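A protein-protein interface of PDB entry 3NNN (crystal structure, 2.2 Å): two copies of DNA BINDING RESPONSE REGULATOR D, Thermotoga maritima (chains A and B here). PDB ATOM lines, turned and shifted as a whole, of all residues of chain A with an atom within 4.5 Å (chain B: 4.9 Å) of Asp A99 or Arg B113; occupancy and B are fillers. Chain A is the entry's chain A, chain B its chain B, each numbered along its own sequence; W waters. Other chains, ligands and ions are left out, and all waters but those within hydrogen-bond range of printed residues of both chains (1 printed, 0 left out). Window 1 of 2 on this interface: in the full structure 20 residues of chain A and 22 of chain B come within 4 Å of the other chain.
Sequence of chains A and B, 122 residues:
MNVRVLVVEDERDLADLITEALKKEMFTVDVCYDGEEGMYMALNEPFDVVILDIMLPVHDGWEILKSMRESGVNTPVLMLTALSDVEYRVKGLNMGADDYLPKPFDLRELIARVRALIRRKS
The side-chain carboxylate of Asp A99 is in salt-bridge range of the guanidinium group of Arg B113 (3.0 Å).
O of Tyr A100 lies within hydrogen-bond range of NH2 of Arg B113.
OD1 of Asp B99 lies within salt-bridge range of NH1 of Arg A113.
The backbone carbonyl oxygen of Val A77 sits at hydrogen-bond distance from the backbone NH of Asp A99 (3.3 Å).
N of Met A79 is in hydrogen-bond range of O of Asp A99 (3.2 Å).
NH1 of Arg A113 lies within salt-bridge range of OD2 of Asp A99 (2.9 Å).
NH1 of Arg B113 lies within salt-bridge range of OD2 of Asp B99, 3.0 Å away.
The side-chain carboxylate (OE2) of Glu B109 lies within salt-bridge range of the guanidinium group (NE) of Arg B113, 2.9 Å away.
Leu A93 touches Arg B113.
Of the printed residues of chain B, Leu A93 touches Arg B113 (3.8 Å).
Asp A99 touches one residue of chain B.
Of the printed residues of chain B, Tyr A100 touches Arg B113.
Of the printed residues of chain B, Arg A113 touches Asp B99.
Of chain A, only Leu A93, Asp A99 and Tyr A100 come within 4 Å of Arg B113.
Leu B117 touches none of the printed residues of chain A.
The nearest residue of chain B that does not touch Asp A99 is Asp B99 (4.4 Å).
The nearest printed residue of chain A that does not touch Asp B99 is Asp A99 (4.4 Å).
Of the 10 printed residues of chain A, 4 touch a printed residue of chain B.
Of the 12 printed residues of chain B, 2 touch a printed residue of chain A.
Among the printed residues, Asp or Glu carboxylates within 4 Å of a Lys or Arg side-chain nitrogen of the other chain: Asp A99 with Arg B113 and Arg A113 with Asp B99.
Asp A99 touches Arg B113, and with the chains exchanged Arg A113 touches Asp B99.
4 positions are printed for both chains.
Of the 4 pairs that touch across the chains among the printed residues, 2 have their exchanged pair printed and touching as well.
Water W1 bridges O of Ala B112 and O of Leu A93.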
ATOM      1  N   VAL A  77      -6.643  13.413 -19.347  1.00  0.00           N
ATOM      2  CA  VAL A  77      -7.926  12.742 -19.307  1.00  0.00           C
ATOM      3  C   VAL A  77      -7.941  11.465 -20.121  1.00  0.00           C
ATOM      4  O   VAL A  77      -7.465  11.425 -21.265  1.00  0.00           O
ATOM      5  CB  VAL A  77      -9.050  13.631 -19.855  1.00  0.00           C
ATOM      6  CG1 VAL A  77     -10.339  12.830 -19.924  1.00  0.00           C
ATOM      7  CG2 VAL A  77      -9.224  14.858 -18.978  1.00  0.00           C
ATOM      8  N   LEU A  78      -8.500  10.422 -19.521  1.00  0.00           N
ATOM      9  CA  LEU A  78      -8.642   9.138 -20.188  1.00  0.00           C
ATOM     10  C   LEU A  78     -10.121   8.796 -20.159  1.00  0.00           C
ATOM     11  O   LEU A  78     -10.738   8.775 -19.097  1.00  0.00           O
ATOM     12  CB  LEU A  78      -7.847   8.046 -19.466  1.00  0.00           C
ATOM     13  CG  LEU A  78      -7.690   6.698 -20.189  1.00  0.00           C
ATOM     14  CD1 LEU A  78      -6.604   5.888 -19.482  1.00  0.00           C
ATOM     15  CD2 LEU A  78      -8.996   5.918 -20.200  1.00  0.00           C
ATOM     16  N   MET A  79     -10.707   8.559 -21.323  1.00  0.00           N
ATOM     17  CA  MET A  79     -12.111   8.197 -21.342  1.00  0.00           C
ATOM     18  C   MET A  79     -12.236   6.669 -21.438  1.00  0.00           C
ATOM     19  O   MET A  79     -11.515   6.031 -22.208  1.00  0.00           O
ATOM     20  CB  MET A  79     -12.818   8.897 -22.510  1.00  0.00           C
ATOM     21  CG  MET A  79     -12.729  10.430 -22.441  1.00  0.00           C
ATOM     22  SD  MET A  79     -13.416  11.245 -23.903  1.00  0.00           S
ATOM     23  CE  MET A  79     -14.672  12.274 -23.168  1.00  0.00           C
ATOM     24  N   LEU A  93     -10.896  12.371 -28.369  1.00  0.00           N
ATOM     25  CA  LEU A  93      -9.530  12.836 -28.529  1.00  0.00           C
ATOM     26  C   LEU A  93      -9.500  14.260 -29.088  1.00  0.00           C
ATOM     27  O   LEU A  93      -8.873  15.144 -28.512  1.00  0.00           O
ATOM     28  CB  LEU A  93      -8.772  11.874 -29.450  1.00  0.00           C
ATOM     29  CG  LEU A  93      -8.536  10.449 -28.908  1.00  0.00           C
ATOM     30  CD1 LEU A  93      -8.373   9.433 -30.058  1.00  0.00           C
ATOM     31  CD2 LEU A  93      -7.304  10.459 -28.017  1.00  0.00           C
ATOM     32  N   ALA A  97      -9.356  14.835 -24.979  1.00  0.00           N
ATOM     33  CA  ALA A  97      -9.017  13.655 -24.196  1.00  0.00           C
ATOM     34  C   ALA A  97      -7.596  13.282 -24.595  1.00  0.00           C
ATOM     35  O   ALA A  97      -7.189  13.503 -25.737  1.00  0.00           O
ATOM     36  CB  ALA A  97      -9.964  12.507 -24.517  1.00  0.00           C
ATOM     37  N   ASP A  98      -6.841  12.723 -23.660  1.00  0.00           N
ATOM     38  CA  ASP A  98      -5.456  12.334 -23.924  1.00  0.00           C
ATOM     39  C   ASP A  98      -5.321  10.889 -24.404  1.00  0.00           C
ATOM     40  O   ASP A  98      -4.326  10.521 -25.026  1.00  0.00           O
ATOM     41  CB  ASP A  98      -4.627  12.603 -22.671  1.00  0.00           C
ATOM     42  CG  ASP A  98      -4.550  14.084 -22.357  1.00  0.00           C
ATOM     43  OD1 ASP A  98      -5.287  14.572 -21.468  1.00  0.00           O
ATOM     44  OD2 ASP A  98      -3.762  14.774 -23.033  1.00  0.00           O
ATOM     45  N   ASP A  99      -6.340  10.085 -24.114  1.00  0.00           N
ATOM     46  CA  ASP A  99      -6.421   8.688 -24.536  1.00  0.00           C
ATOM     47  C   ASP A  99      -7.895   8.309 -24.424  1.00  0.00           C
ATOM     48  O   ASP A  99      -8.670   8.963 -23.721  1.00  0.00           O
ATOM     49  CB  ASP A  99      -5.577   7.753 -23.661  1.00  0.00           C
ATOM     50  CG  ASP A  99      -5.274   6.419 -24.354  1.00  0.00           C
ATOM     51  OD1 ASP A  99      -6.027   6.012 -25.278  1.00  0.00           O
ATOM     52  OD2 ASP A  99      -4.281   5.765 -23.972  1.00  0.00           O
ATOM     53  N   TYR A 100      -8.263   7.246 -25.128  1.00  0.00           N
ATOM     54  CA  TYR A 100      -9.633   6.766 -25.196  1.00  0.00           C
ATOM     55  C   TYR A 100      -9.574   5.244 -25.239  1.00  0.00           C
ATOM     56  O   TYR A 100      -9.028   4.665 -26.181  1.00  0.00           O
ATOM     57  CB  TYR A 100     -10.274   7.298 -26.484  1.00  0.00           C
ATOM     58  CG  TYR A 100     -11.785   7.258 -26.542  1.00  0.00           C
ATOM     59  CD1 TYR A 100     -12.533   8.419 -26.347  1.00  0.00           C
ATOM     60  CD2 TYR A 100     -12.470   6.073 -26.820  1.00  0.00           C
ATOM     61  CE1 TYR A 100     -13.925   8.408 -26.430  1.00  0.00           C
ATOM     62  CE2 TYR A 100     -13.875   6.052 -26.902  1.00  0.00           C
ATOM     63  CZ  TYR A 100     -14.590   7.231 -26.702  1.00  0.00           C
ATOM     64  OH  TYR A 100     -15.967   7.235 -26.743  1.00  0.00           O
ATOM     65  N   LEU A 101     -10.123   4.602 -24.215  1.00  0.00           N
ATOM     66  CA  LEU A 101     -10.118   3.153 -24.128  1.00  0.00           C
ATOM     67  C   LEU A 101     -11.548   2.650 -23.989  1.00  0.00           C
ATOM     68  O   LEU A 101     -12.196   2.823 -22.956  1.00  0.00           O
ATOM     69  CB  LEU A 101      -9.278   2.706 -22.925  1.00  0.00           C
ATOM     70  CG  LEU A 101      -9.017   1.209 -22.744  1.00  0.00           C
ATOM     71  CD1 LEU A 101      -8.240   0.695 -23.936  1.00  0.00           C
ATOM     72  CD2 LEU A 101      -8.216   0.962 -21.465  1.00  0.00           C
ATOM     73  N   ARG A 113      -2.059   2.297 -19.450  1.00  0.00           N
ATOM     74  CA  ARG A 113      -2.333   3.596 -20.082  1.00  0.00           C
ATOM     75  C   ARG A 113      -2.431   4.743 -19.091  1.00  0.00           C
ATOM     76  O   ARG A 113      -2.083   5.881 -19.410  1.00  0.00           O
ATOM     77  CB  ARG A 113      -3.605   3.528 -20.942  1.00  0.00           C
ATOM     78  CG  ARG A 113      -3.402   2.739 -22.228  1.00  0.00           C
ATOM     79  CD  ARG A 113      -4.668   2.620 -23.090  1.00  0.00           C
ATOM     80  NE  ARG A 113      -4.423   1.806 -24.283  1.00  0.00           N
ATOM     81  CZ  ARG A 113      -3.826   2.239 -25.395  1.00  0.00           C
ATOM     82  NH1 ARG A 113      -3.412   3.494 -25.497  1.00  0.00           N
ATOM     83  NH2 ARG A 113      -3.615   1.400 -26.403  1.00  0.00           N
ATOM     84  N   LEU B  78       4.371   6.793 -30.531  1.00  0.00           N
ATOM     85  CA  LEU B  78       3.164   6.055 -30.827  1.00  0.00           C
ATOM     86  C   LEU B  78       3.611   4.792 -31.547  1.00  0.00           C
ATOM     87  O   LEU B  78       4.325   4.861 -32.551  1.00  0.00           O
ATOM     88  CB  LEU B  78       2.240   6.867 -31.735  1.00  0.00           C
ATOM     89  CG  LEU B  78       1.089   6.069 -32.365  1.00  0.00           C
ATOM     90  CD1 LEU B  78       0.172   5.551 -31.286  1.00  0.00           C
ATOM     91  CD2 LEU B  78       0.319   6.957 -33.317  1.00  0.00           C
ATOM     92  N   ASP B  99       1.575   5.808 -26.585  1.00  0.00           N
ATOM     93  CA  ASP B  99       0.344   5.263 -27.119  1.00  0.00           C
ATOM     94  C   ASP B  99       0.749   4.064 -27.946  1.00  0.00           C
ATOM     95  O   ASP B  99       1.900   3.935 -28.362  1.00  0.00           O
ATOM     96  CB  ASP B  99      -0.408   6.274 -27.993  1.00  0.00           C
ATOM     97  CG  ASP B  99      -1.893   5.953 -28.102  1.00  0.00           C
ATOM     98  OD1 ASP B  99      -2.287   4.803 -27.779  1.00  0.00           O
ATOM     99  OD2 ASP B  99      -2.674   6.849 -28.511  1.00  0.00           O
ATOM    100  N   LEU B 101      -1.053   1.686 -31.083  1.00  0.00           N
ATOM    101  CA  LEU B 101      -2.188   1.456 -31.973  1.00  0.00           C
ATOM    102  C   LEU B 101      -1.871   0.288 -32.902  1.00  0.00           C
ATOM    103  O   LEU B 101      -0.875   0.305 -33.624  1.00  0.00           O
ATOM    104  CB  LEU B 101      -2.484   2.717 -32.805  1.00  0.00           C
ATOM    105  CG  LEU B 101      -3.774   2.739 -33.648  1.00  0.00           C
ATOM    106  CD1 LEU B 101      -4.965   2.650 -32.714  1.00  0.00           C
ATOM    107  CD2 LEU B 101      -3.869   4.023 -34.494  1.00  0.00           C
ATOM    108  N   GLU B 109      -8.269   7.776 -36.605  1.00  0.00           N
ATOM    109  CA  GLU B 109      -7.833   7.571 -35.234  1.00  0.00           C
ATOM    110  C   GLU B 109      -6.325   7.812 -35.087  1.00  0.00           C
ATOM    111  O   GLU B 109      -5.878   8.306 -34.055  1.00  0.00           O
ATOM    112  CB  GLU B 109      -8.219   6.166 -34.756  1.00  0.00           C
ATOM    113  CG  GLU B 109      -7.682   5.840 -33.372  1.00  0.00           C
ATOM    114  CD  GLU B 109      -8.409   4.703 -32.690  1.00  0.00           C
ATOM    115  OE1 GLU B 109      -8.872   3.768 -33.377  1.00  0.00           O
ATOM    116  OE2 GLU B 109      -8.504   4.742 -31.449  1.00  0.00           O
ATOM    117  N   LEU B 110      -5.543   7.485 -36.120  1.00  0.00           N
ATOM    118  CA  LEU B 110      -4.089   7.688 -36.072  1.00  0.00           C
ATOM    119  C   LEU B 110      -3.686   9.154 -35.917  1.00  0.00           C
ATOM    120  O   LEU B 110      -2.886   9.489 -35.034  1.00  0.00           O
ATOM    121  CB  LEU B 110      -3.400   7.118 -37.320  1.00  0.00           C
ATOM    122  CG  LEU B 110      -1.915   7.522 -37.471  1.00  0.00           C
ATOM    123  CD1 LEU B 110      -1.132   7.034 -36.261  1.00  0.00           C
ATOM    124  CD2 LEU B 110      -1.311   6.944 -38.763  1.00  0.00           C
ATOM    125  N   ILE B 111      -4.209  10.035 -36.771  1.00  0.00           N
ATOM    126  CA  ILE B 111      -3.833  11.447 -36.640  1.00  0.00           C
ATOM    127  C   ILE B 111      -4.525  12.079 -35.427  1.00  0.00           C
ATOM    128  O   ILE B 111      -4.013  13.025 -34.847  1.00  0.00           O
ATOM    129  CB  ILE B 111      -4.133  12.284 -37.929  1.00  0.00           C
ATOM    130  CG1 ILE B 111      -5.616  12.577 -38.044  1.00  0.00           C
ATOM    131  CG2 ILE B 111      -3.649  11.533 -39.176  1.00  0.00           C
ATOM    132  CD1 ILE B 111      -6.422  11.372 -38.378  1.00  0.00           C
ATOM    133  N   ALA B 112      -5.677  11.549 -35.029  1.00  0.00           N
ATOM    134  CA  ALA B 112      -6.347  12.093 -33.855  1.00  0.00           C
ATOM    135  C   ALA B 112      -5.437  11.839 -32.653  1.00  0.00           C
ATOM    136  O   ALA B 112      -5.215  12.726 -31.832  1.00  0.00           O
ATOM    137  CB  ALA B 112      -7.695  11.425 -33.646  1.00  0.00           C
ATOM    138  N   ARG B 113      -4.905  10.622 -32.556  1.00  0.00           N
ATOM    139  CA  ARG B 113      -4.020  10.264 -31.455  1.00  0.00           C
ATOM    140  C   ARG B 113      -2.693  11.001 -31.549  1.00  0.00           C
ATOM    141  O   ARG B 113      -2.125  11.413 -30.540  1.00  0.00           O
ATOM    142  CB  ARG B 113      -3.782   8.746 -31.439  1.00  0.00           C
ATOM    143  CG  ARG B 113      -4.993   7.981 -30.944  1.00  0.00           C
ATOM    144  CD  ARG B 113      -4.818   6.481 -30.945  1.00  0.00           C
ATOM    145  NE  ARG B 113      -6.047   5.869 -30.432  1.00  0.00           N
ATOM    146  CZ  ARG B 113      -6.381   5.833 -29.146  1.00  0.00           C
ATOM    147  NH1 ARG B 113      -5.570   6.352 -28.229  1.00  0.00           N
ATOM    148  NH2 ARG B 113      -7.545   5.328 -28.780  1.00  0.00           N
ATOM    149  N   VAL B 114      -2.198  11.159 -32.770  1.00  0.00           N
ATOM    150  CA  VAL B 114      -0.942  11.853 -32.997  1.00  0.00           C
ATOM    151  C   VAL B 114      -1.018  13.302 -32.515  1.00  0.00           C
ATOM    152  O   VAL B 114      -0.128  13.781 -31.815  1.00  0.00           O
ATOM    153  CB  VAL B 114      -0.566  11.813 -34.492  1.00  0.00           C
ATOM    154  CG1 VAL B 114       0.454  12.907 -34.816  1.00  0.00           C
ATOM    155  CG2 VAL B 114       0.019  10.431 -34.830  1.00  0.00           C
ATOM    156  N   ARG B 115      -2.084  13.999 -32.879  1.00  0.00           N
ATOM    157  CA  ARG B 115      -2.203  15.372 -32.450  1.00  0.00           C
ATOM    158  C   ARG B 115      -2.418  15.464 -30.946  1.00  0.00           C
ATOM    159  O   ARG B 115      -1.937  16.398 -30.301  1.00  0.00           O
ATOM    160  CB  ARG B 115      -3.327  16.081 -33.200  1.00  0.00           C
ATOM    161  CG  ARG B 115      -4.703  15.528 -32.971  1.00  0.00           C
ATOM    162  CD  ARG B 115      -5.724  16.588 -33.357  1.00  0.00           C
ATOM    163  NE  ARG B 115      -5.499  17.069 -34.716  1.00  0.00           N
ATOM    164  CZ  ARG B 115      -5.788  18.298 -35.130  1.00  0.00           C
ATOM    165  NH1 ARG B 115      -6.314  19.181 -34.285  1.00  0.00           N
ATOM    166  NH2 ARG B 115      -5.547  18.645 -36.390  1.00  0.00           N
ATOM    167  N   ALA B 116      -3.129  14.493 -30.378  1.00  0.00           N
ATOM    168  CA  ALA B 116      -3.355  14.495 -28.934  1.00  0.00           C
ATOM    169  C   ALA B 116      -2.014  14.329 -28.200  1.00  0.00           C
ATOM    170  O   ALA B 116      -1.806  14.921 -27.139  1.00  0.00           O
ATOM    171  CB  ALA B 116      -4.323  13.373 -28.535  1.00  0.00           C
ATOM    172  N   LEU B 117      -1.105  13.532 -28.764  1.00  0.00           N
ATOM    173  CA  LEU B 117       0.201  13.330 -28.135  1.00  0.00           C
ATOM    174  C   LEU B 117       1.056  14.604 -28.165  1.00  0.00           C
ATOM    175  O   LEU B 117       1.593  15.022 -27.142  1.00  0.00           O
ATOM    176  CB  LEU B 117       0.968  12.185 -28.810  1.00  0.00           C
ATOM    177  CG  LEU B 117       0.508  10.751 -28.501  1.00  0.00           C
ATOM    178  CD1 LEU B 117       1.248   9.763 -29.407  1.00  0.00           C
ATOM    179  CD2 LEU B 117       0.767  10.423 -27.040  1.00  0.00           C
HETATM  180  O   HOH W   1      -7.205  14.784 -31.334  1.00  0.00           O
